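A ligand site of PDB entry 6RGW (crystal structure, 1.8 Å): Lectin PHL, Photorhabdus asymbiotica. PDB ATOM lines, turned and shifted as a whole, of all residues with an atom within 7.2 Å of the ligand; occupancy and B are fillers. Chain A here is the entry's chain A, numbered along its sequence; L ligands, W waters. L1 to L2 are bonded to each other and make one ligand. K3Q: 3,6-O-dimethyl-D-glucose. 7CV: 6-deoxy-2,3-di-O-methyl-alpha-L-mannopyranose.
CB of Lys 75 touches O2 of 7CV L2, 3.7 Å away.
Val 78 touches the ligand.
Gly 98 touches the ligand.
Trp 104 touches the ligand.
CE3 of Trp 118 touches C8 of K3Q L1 (3.5 Å).
Hydrophobic or aromatic side chains that line the ligand: Val 78, Trp 104 and Trp 118.
Within 4 Å of the ligand: Lys 75, Gly 76, Gln 77, Val 78, Gly 98, Thr 99, Asp 100, Trp 104 and Trp 118.
The nearest printed residue that does not touch the ligand is Ala 53 (5.1 Å).
O of Gln 77 sits at hydrogen-bond distance from N of Thr 99, at 3.2 Å.
O of Asp 51 lies within hydrogen-bond range of NE2 of Gln 77 (2.7 Å).
OD1 of Asp 100 lies within hydrogen-bond range of NE1 of Trp 104 (3.0 Å).
The indole nitrogen of Trp 118 lies within hydrogen-bond range of the backbone carbonyl oxygen of Lys 75, at 3.5 Å.
The backbone carbonyl oxygen (O) of Gly 98 sits at hydrogen-bond distance from the side-chain hydroxyl (OG1) of Thr 79.
The backbone carbonyl oxygen (O) of Ala 96 sits at hydrogen-bond distance from the backbone NH (N) of Trp 104, at 2.8 Å.
The side-chain hydroxyl (OG) of Ser 73 lies within hydrogen-bond range of the backbone NH (N) of Lys 75 (2.8 Å).
N of Val 78 is in hydrogen-bond range of O of Lys 52 (2.9 Å).
An oxygen (O6) of K3Q L1 sits at hydrogen-bond distance from the backbone NH (N) of Gln 77, 2.9 Å away.
N of Thr 99 is in hydrogen-bond range of O4 of K3Q L1 (3.0 Å).
The side-chain hydroxyl (OG1) of Thr 99 lies within hydrogen-bond range of an oxygen (O4) of K3Q L1, at 2.9 Å.
N of Gly 76 lies within hydrogen-bond range of O2 of 7CV L2 (3.0 Å).
N of Asp 100 is in hydrogen-bond range of O4 of K3Q L1 (3.2 Å).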
ATOM      1  N   ASP A  51     -17.593 -21.355  22.180  1.00  0.00           N
ATOM      2  CA  ASP A  51     -18.248 -22.335  21.273  1.00  0.00           C
ATOM      3  C   ASP A  51     -19.698 -21.913  20.979  1.00  0.00           C
ATOM      4  O   ASP A  51     -20.354 -22.635  20.215  1.00  0.00           O
ATOM      5  CB  ASP A  51     -18.177 -23.749  21.859  1.00  0.00           C
ATOM      6  CG  ASP A  51     -18.845 -23.948  23.221  1.00  0.00           C
ATOM      7  OD1 ASP A  51     -19.090 -22.924  23.921  1.00  0.00           O
ATOM      8  OD2 ASP A  51     -19.096 -25.128  23.588  1.00  0.00           O
ATOM      9  N   LYS A  52     -20.165 -20.794  21.553  1.00  0.00           N
ATOM     10  CA  LYS A  52     -21.532 -20.231  21.360  1.00  0.00           C
ATOM     11  C   LYS A  52     -22.589 -21.139  22.026  1.00  0.00           C
ATOM     12  O   LYS A  52     -23.788 -20.909  21.772  1.00  0.00           O
ATOM     13  CB  LYS A  52     -21.848 -20.015  19.879  1.00  0.00           C
ATOM     14  CG  LYS A  52     -20.901 -19.046  19.187  1.00  0.00           C
ATOM     15  CD  LYS A  52     -21.454 -18.440  17.917  1.00  0.00           C
ATOM     16  CE  LYS A  52     -20.414 -17.597  17.210  1.00  0.00           C
ATOM     17  NZ  LYS A  52     -20.899 -17.078  15.914  1.00  0.00           N
ATOM     18  N   ALA A  53     -22.166 -22.088  22.875  1.00  0.00           N
ATOM     19  CA  ALA A  53     -23.105 -22.877  23.708  1.00  0.00           C
ATOM     20  C   ALA A  53     -23.437 -22.083  24.977  1.00  0.00           C
ATOM     21  O   ALA A  53     -22.671 -21.180  25.345  1.00  0.00           O
ATOM     22  CB  ALA A  53     -22.518 -24.225  24.057  1.00  0.00           C
ATOM     23  N   VAL A  54     -24.569 -22.398  25.591  1.00  0.00           N
ATOM     24  CA  VAL A  54     -24.960 -21.830  26.904  1.00  0.00           C
ATOM     25  C   VAL A  54     -24.351 -22.733  27.966  1.00  0.00           C
ATOM     26  O   VAL A  54     -24.530 -23.958  27.863  1.00  0.00           O
ATOM     27  CB  VAL A  54     -26.492 -21.706  27.040  1.00  0.00           C
ATOM     28  CG1 VAL A  54     -26.874 -21.185  28.414  1.00  0.00           C
ATOM     29  CG2 VAL A  54     -27.084 -20.829  25.944  1.00  0.00           C
ATOM     30  N   SER A  73     -22.118 -27.421  30.187  1.00  0.00           N
ATOM     31  CA  SER A  73     -22.757 -26.943  28.935  1.00  0.00           C
ATOM     32  C   SER A  73     -24.202 -27.429  28.857  1.00  0.00           C
ATOM     33  O   SER A  73     -24.465 -28.626  29.121  1.00  0.00           O
ATOM     34  CB  SER A  73     -21.963 -27.391  27.739  1.00  0.00           C
ATOM     35  OG  SER A  73     -22.627 -26.984  26.551  1.00  0.00           O
ATOM     36  N   LEU A  74     -25.117 -26.538  28.494  1.00  0.00           N
ATOM     37  CA  LEU A  74     -26.501 -26.884  28.076  1.00  0.00           C
ATOM     38  C   LEU A  74     -26.536 -26.997  26.552  1.00  0.00           C
ATOM     39  O   LEU A  74     -27.627 -27.237  26.002  1.00  0.00           O
ATOM     40  CB  LEU A  74     -27.469 -25.798  28.560  1.00  0.00           C
ATOM     41  CG  LEU A  74     -27.612 -25.665  30.075  1.00  0.00           C
ATOM     42  CD1 LEU A  74     -28.593 -24.548  30.417  1.00  0.00           C
ATOM     43  CD2 LEU A  74     -28.051 -26.971  30.706  1.00  0.00           C
ATOM     44  N   LYS A  75     -25.381 -26.838  25.888  1.00  0.00           N
ATOM     45  CA  LYS A  75     -25.250 -26.899  24.408  1.00  0.00           C
ATOM     46  C   LYS A  75     -26.041 -25.745  23.792  1.00  0.00           C
ATOM     47  O   LYS A  75     -26.097 -24.669  24.419  1.00  0.00           O
ATOM     48  CB  LYS A  75     -25.696 -28.277  23.897  1.00  0.00           C
ATOM     49  CG  LYS A  75     -24.966 -29.470  24.507  1.00  0.00           C
ATOM     50  CD  LYS A  75     -25.602 -30.792  24.133  1.00  0.00           C
ATOM     51  CE  LYS A  75     -24.624 -31.946  24.106  1.00  0.00           C
ATOM     52  NZ  LYS A  75     -25.284 -33.211  23.712  1.00  0.00           N
ATOM     53  N   GLY A  76     -26.622 -25.953  22.612  1.00  0.00           N
ATOM     54  CA  GLY A  76     -27.236 -24.882  21.806  1.00  0.00           C
ATOM     55  C   GLY A  76     -26.174 -24.052  21.115  1.00  0.00           C
ATOM     56  O   GLY A  76     -24.978 -24.237  21.395  1.00  0.00           O
ATOM     57  N   GLN A  77     -26.607 -23.176  20.207  1.00  0.00           N
ATOM     58  CA  GLN A  77     -25.736 -22.212  19.491  1.00  0.00           C
ATOM     59  C   GLN A  77     -26.517 -20.903  19.475  1.00  0.00           C
ATOM     60  O   GLN A  77     -27.558 -20.848  18.794  1.00  0.00           O
ATOM     61  CB  GLN A  77     -25.396 -22.729  18.082  1.00  0.00           C
ATOM     62  CG  GLN A  77     -24.492 -23.956  18.095  1.00  0.00           C
ATOM     63  CD  GLN A  77     -23.071 -23.624  18.481  1.00  0.00           C
ATOM     64  OE1 GLN A  77     -22.276 -23.187  17.646  1.00  0.00           O
ATOM     65  NE2 GLN A  77     -22.731 -23.846  19.739  1.00  0.00           N
ATOM     66  N   VAL A  78     -26.081 -19.921  20.271  1.00  0.00           N
ATOM     67  CA  VAL A  78     -26.889 -18.720  20.587  1.00  0.00           C
ATOM     68  C   VAL A  78     -26.166 -17.457  20.114  1.00  0.00           C
ATOM     69  O   VAL A  78     -24.907 -17.435  20.125  1.00  0.00           O
ATOM     70  CB  VAL A  78     -27.241 -18.638  22.087  1.00  0.00           C
ATOM     71  CG1 VAL A  78     -27.986 -19.878  22.540  1.00  0.00           C
ATOM     72  CG2 VAL A  78     -26.029 -18.388  22.967  1.00  0.00           C
ATOM     73  N   THR A  79     -26.955 -16.435  19.780  1.00  0.00           N
ATOM     74  CA  THR A  79     -26.513 -15.094  19.313  1.00  0.00           C
ATOM     75  C   THR A  79     -27.189 -13.993  20.146  1.00  0.00           C
ATOM     76  O   THR A  79     -27.309 -12.850  19.648  1.00  0.00           O
ATOM     77  CB  THR A  79     -26.781 -14.972  17.815  1.00  0.00           C
ATOM     78  OG1 THR A  79     -28.194 -15.106  17.610  1.00  0.00           O
ATOM     79  CG2 THR A  79     -26.052 -16.016  17.004  1.00  0.00           C
ATOM     80  N   ALA A  96     -33.025 -17.706  24.586  1.00  0.00           N
ATOM     81  CA  ALA A  96     -31.889 -17.174  23.822  1.00  0.00           C
ATOM     82  C   ALA A  96     -32.254 -17.094  22.340  1.00  0.00           C
ATOM     83  O   ALA A  96     -33.005 -17.970  21.865  1.00  0.00           O
ATOM     84  CB  ALA A  96     -30.675 -18.038  24.027  1.00  0.00           C
ATOM     85  N   ARG A  97     -31.689 -16.113  21.643  1.00  0.00           N
ATOM     86  CA  ARG A  97     -31.710 -16.104  20.162  1.00  0.00           C
ATOM     87  C   ARG A  97     -30.751 -17.175  19.664  1.00  0.00           C
ATOM     88  O   ARG A  97     -29.621 -17.250  20.201  1.00  0.00           O
ATOM     89  CB  ARG A  97     -31.332 -14.738  19.594  1.00  0.00           C
ATOM     90  CG  ARG A  97     -31.563 -14.644  18.104  1.00  0.00           C
ATOM     91  CD  ARG A  97     -31.286 -13.256  17.568  1.00  0.00           C
ATOM     92  NE  ARG A  97     -29.876 -12.899  17.659  1.00  0.00           N
ATOM     93  CZ  ARG A  97     -29.349 -11.801  17.139  1.00  0.00           C
ATOM     94  NH1 ARG A  97     -30.116 -10.949  16.472  1.00  0.00           N
ATOM     95  NH2 ARG A  97     -28.062 -11.550  17.277  1.00  0.00           N
ATOM     96  N   GLY A  98     -31.187 -17.983  18.699  1.00  0.00           N
ATOM     97  CA  GLY A  98     -30.370 -18.999  18.027  1.00  0.00           C
ATOM     98  C   GLY A  98     -29.575 -18.359  16.898  1.00  0.00           C
ATOM     99  O   GLY A  98     -29.853 -17.209  16.547  1.00  0.00           O
ATOM    100  N   THR A  99     -28.578 -19.075  16.372  1.00  0.00           N
ATOM    101  CA  THR A  99     -27.811 -18.664  15.163  1.00  0.00           C
ATOM    102  C   THR A  99     -28.774 -18.491  13.981  1.00  0.00           C
ATOM    103  O   THR A  99     -28.383 -17.757  13.042  1.00  0.00           O
ATOM    104  CB  THR A  99     -26.655 -19.643  14.904  1.00  0.00           C
ATOM    105  OG1 THR A  99     -27.169 -20.976  14.932  1.00  0.00           O
ATOM    106  CG2 THR A  99     -25.529 -19.516  15.909  1.00  0.00           C
ATOM    107  N   ASP A 100     -29.966 -19.085  14.021  1.00  0.00           N
ATOM    108  CA  ASP A 100     -31.015 -18.931  12.970  1.00  0.00           C
ATOM    109  C   ASP A 100     -31.902 -17.695  13.227  1.00  0.00           C
ATOM    110  O   ASP A 100     -32.858 -17.500  12.459  1.00  0.00           O
ATOM    111  CB  ASP A 100     -31.863 -20.199  12.820  1.00  0.00           C
ATOM    112  CG  ASP A 100     -32.726 -20.528  14.025  1.00  0.00           C
ATOM    113  OD1 ASP A 100     -32.605 -19.801  15.039  1.00  0.00           O
ATOM    114  OD2 ASP A 100     -33.507 -21.488  13.934  1.00  0.00           O
ATOM    115  N   ASN A 101     -31.600 -16.912  14.269  1.00  0.00           N
ATOM    116  CA  ASN A 101     -32.306 -15.665  14.670  1.00  0.00           C
ATOM    117  C   ASN A 101     -33.721 -15.951  15.212  1.00  0.00           C
ATOM    118  O   ASN A 101     -34.453 -14.973  15.474  1.00  0.00           O
ATOM    119  CB  ASN A 101     -32.339 -14.649  13.531  1.00  0.00           C
ATOM    120  CG  ASN A 101     -30.980 -14.056  13.287  1.00  0.00           C
ATOM    121  OD1 ASN A 101     -30.325 -13.605  14.228  1.00  0.00           O
ATOM    122  ND2 ASN A 101     -30.528 -14.079  12.038  1.00  0.00           N
ATOM    123  N   ALA A 102     -34.101 -17.206  15.413  1.00  0.00           N
ATOM    124  CA  ALA A 102     -35.367 -17.546  16.104  1.00  0.00           C
ATOM    125  C   ALA A 102     -35.168 -17.433  17.611  1.00  0.00           C
ATOM    126  O   ALA A 102     -34.010 -17.377  18.096  1.00  0.00           O
ATOM    127  CB  ALA A 102     -35.866 -18.900  15.696  1.00  0.00           C
ATOM    128  N   LEU A 103     -36.274 -17.366  18.349  1.00  0.00           N
ATOM    129  CA  LEU A 103     -36.259 -17.514  19.817  1.00  0.00           C
ATOM    130  C   LEU A 103     -36.229 -19.011  20.120  1.00  0.00           C
ATOM    131  O   LEU A 103     -37.094 -19.751  19.615  1.00  0.00           O
ATOM    132  CB  LEU A 103     -37.488 -16.841  20.440  1.00  0.00           C
ATOM    133  CG  LEU A 103     -37.645 -17.092  21.943  1.00  0.00           C
ATOM    134  CD1 LEU A 103     -36.525 -16.432  22.717  1.00  0.00           C
ATOM    135  CD2 LEU A 103     -39.004 -16.602  22.429  1.00  0.00           C
ATOM    136  N   TRP A 104     -35.256 -19.416  20.935  1.00  0.00           N
ATOM    137  CA  TRP A 104     -35.121 -20.812  21.413  1.00  0.00           C
ATOM    138  C   TRP A 104     -35.299 -20.822  22.933  1.00  0.00           C
ATOM    139  O   TRP A 104     -35.039 -19.797  23.582  1.00  0.00           O
ATOM    140  CB  TRP A 104     -33.758 -21.391  21.017  1.00  0.00           C
ATOM    141  CG  TRP A 104     -33.649 -21.701  19.554  1.00  0.00           C
ATOM    142  CD1 TRP A 104     -33.478 -20.811  18.546  1.00  0.00           C
ATOM    143  CD2 TRP A 104     -33.723 -22.996  18.947  1.00  0.00           C
ATOM    144  NE1 TRP A 104     -33.431 -21.464  17.347  1.00  0.00           N
ATOM    145  CE2 TRP A 104     -33.579 -22.805  17.552  1.00  0.00           C
ATOM    146  CE3 TRP A 104     -33.884 -24.306  19.427  1.00  0.00           C
ATOM    147  CZ2 TRP A 104     -33.591 -23.873  16.650  1.00  0.00           C
ATOM    148  CZ3 TRP A 104     -33.897 -25.358  18.534  1.00  0.00           C
ATOM    149  CH2 TRP A 104     -33.747 -25.143  17.166  1.00  0.00           C
ATOM    150  N   HIS A 105     -35.682 -21.966  23.481  1.00  0.00           N
ATOM    151  CA  HIS A 105     -35.745 -22.115  24.954  1.00  0.00           C
ATOM    152  C   HIS A 105     -35.429 -23.557  25.344  1.00  0.00           C
ATOM    153  O   HIS A 105     -35.502 -24.449  24.489  1.00  0.00           O
ATOM    154  CB  HIS A 105     -37.079 -21.585  25.500  1.00  0.00           C
ATOM    155  CG  HIS A 105     -38.275 -22.379  25.124  1.00  0.00           C
ATOM    156  ND1 HIS A 105     -39.294 -22.631  26.019  1.00  0.00           N
ATOM    157  CD2 HIS A 105     -38.636 -22.984  23.972  1.00  0.00           C
ATOM    158  CE1 HIS A 105     -40.231 -23.346  25.436  1.00  0.00           C
ATOM    159  NE2 HIS A 105     -39.845 -23.582  24.168  1.00  0.00           N
ATOM    160  N   ASN A 117     -34.551 -30.812  25.874  1.00  0.00           N
ATOM    161  CA  ASN A 117     -33.742 -30.395  24.696  1.00  0.00           C
ATOM    162  C   ASN A 117     -34.143 -28.958  24.352  1.00  0.00           C
ATOM    163  O   ASN A 117     -35.257 -28.531  24.752  1.00  0.00           O
ATOM    164  CB  ASN A 117     -33.906 -31.346  23.521  1.00  0.00           C
ATOM    165  CG  ASN A 117     -33.296 -32.702  23.803  1.00  0.00           C
ATOM    166  OD1 ASN A 117     -32.127 -32.798  24.156  1.00  0.00           O
ATOM    167  ND2 ASN A 117     -34.093 -33.744  23.681  1.00  0.00           N
ATOM    168  N   TRP A 118     -33.252 -28.244  23.670  1.00  0.00           N
ATOM    169  CA  TRP A 118     -33.573 -26.919  23.085  1.00  0.00           C
ATOM    170  C   TRP A 118     -34.746 -27.094  22.124  1.00  0.00           C
ATOM    171  O   TRP A 118     -34.764 -28.088  21.375  1.00  0.00           O
ATOM    172  CB  TRP A 118     -32.355 -26.334  22.376  1.00  0.00           C
ATOM    173  CG  TRP A 118     -31.323 -25.774  23.297  1.00  0.00           C
ATOM    174  CD1 TRP A 118     -30.178 -26.372  23.740  1.00  0.00           C
ATOM    175  CD2 TRP A 118     -31.335 -24.454  23.872  1.00  0.00           C
ATOM    176  NE1 TRP A 118     -29.472 -25.511  24.534  1.00  0.00           N
ATOM    177  CE2 TRP A 118     -30.163 -24.335  24.648  1.00  0.00           C
ATOM    178  CE3 TRP A 118     -32.216 -23.368  23.817  1.00  0.00           C
ATOM    179  CZ2 TRP A 118     -29.855 -23.174  25.344  1.00  0.00           C
ATOM    180  CZ3 TRP A 118     -31.915 -22.220  24.511  1.00  0.00           C
ATOM    181  CH2 TRP A 118     -30.741 -22.128  25.253  1.00  0.00           C
ATOM    182  N   GLN A 119     -35.711 -26.175  22.169  1.00  0.00           N
ATOM    183  CA  GLN A 119     -36.875 -26.147  21.260  1.00  0.00           C
ATOM    184  C   GLN A 119     -36.996 -24.720  20.705  1.00  0.00           C
ATOM    185  O   GLN A 119     -36.727 -23.773  21.447  1.00  0.00           O
ATOM    186  CB  GLN A 119     -38.135 -26.619  21.999  1.00  0.00           C
ATOM    187  CG  GLN A 119     -39.428 -26.465  21.204  1.00  0.00           C
ATOM    188  CD  GLN A 119     -40.668 -26.548  22.056  1.00  0.00           C
ATOM    189  OE1 GLN A 119     -41.219 -25.540  22.500  1.00  0.00           O
ATOM    190  NE2 GLN A 119     -41.120 -27.771  22.286  1.00  0.00           N
HETATM  191  C1  K3Q L   1     -28.526 -25.583  16.785  1.00  0.00           C
HETATM  192  C2  K3Q L   1     -29.193 -25.458  15.426  1.00  0.00           C
HETATM  193  O2  K3Q L   1     -28.478 -26.208  14.442  1.00  0.00           O
HETATM  194  O5  K3Q L   1     -29.309 -24.873  17.739  1.00  0.00           O
HETATM  195  C5  K3Q L   1     -29.313 -23.465  17.503  1.00  0.00           C
HETATM  196  C4  K3Q L   1     -29.919 -23.159  16.123  1.00  0.00           C
HETATM  197  O4  K3Q L   1     -29.815 -21.769  15.815  1.00  0.00           O
HETATM  198  C3  K3Q L   1     -29.212 -23.982  15.033  1.00  0.00           C
HETATM  199  O3  K3Q L   1     -29.860 -23.844  13.770  1.00  0.00           O
HETATM  200  C6  K3Q L   1     -30.095 -22.821  18.645  1.00  0.00           C
HETATM  201  O6  K3Q L   1     -29.439 -23.113  19.887  1.00  0.00           O
HETATM  202  C7  K3Q L   1     -28.998 -23.284  12.769  1.00  0.00           C
HETATM  203  C8  K3Q L   1     -30.226 -22.753  21.016  1.00  0.00           C
HETATM  204  C1  7CV L   2     -27.080 -29.397  20.139  1.00  0.00           C
HETATM  205  C2  7CV L   2     -26.069 -28.531  19.390  1.00  0.00           C
HETATM  206  C3  7CV L   2     -26.700 -27.941  18.116  1.00  0.00           C
HETATM  207  C4  7CV L   2     -28.018 -27.251  18.437  1.00  0.00           C
HETATM  208  C5  7CV L   2     -28.942 -28.173  19.248  1.00  0.00           C
HETATM  209  C6  7CV L   2     -30.233 -27.475  19.629  1.00  0.00           C
HETATM  210  O2  7CV L   2     -25.630 -27.497  20.294  1.00  0.00           O
HETATM  211  O3  7CV L   2     -25.806 -27.027  17.479  1.00  0.00           O
HETATM  212  O4  7CV L   2     -28.708 -26.867  17.228  1.00  0.00           O
HETATM  213  O5  7CV L   2     -28.254 -28.624  20.434  1.00  0.00           O
HETATM  214  C24 7CV L   2     -24.211 -27.321  20.425  1.00  0.00           C
HETATM  215  C27 7CV L   2     -24.557 -27.601  17.061  1.00  0.00           C
HETATM  216  O1  7CV L   2     -27.430 -30.546  19.357  1.00  0.00           O
HETATM  217  O   HOH W   1     -32.697 -25.831  13.389  1.00  0.00           O
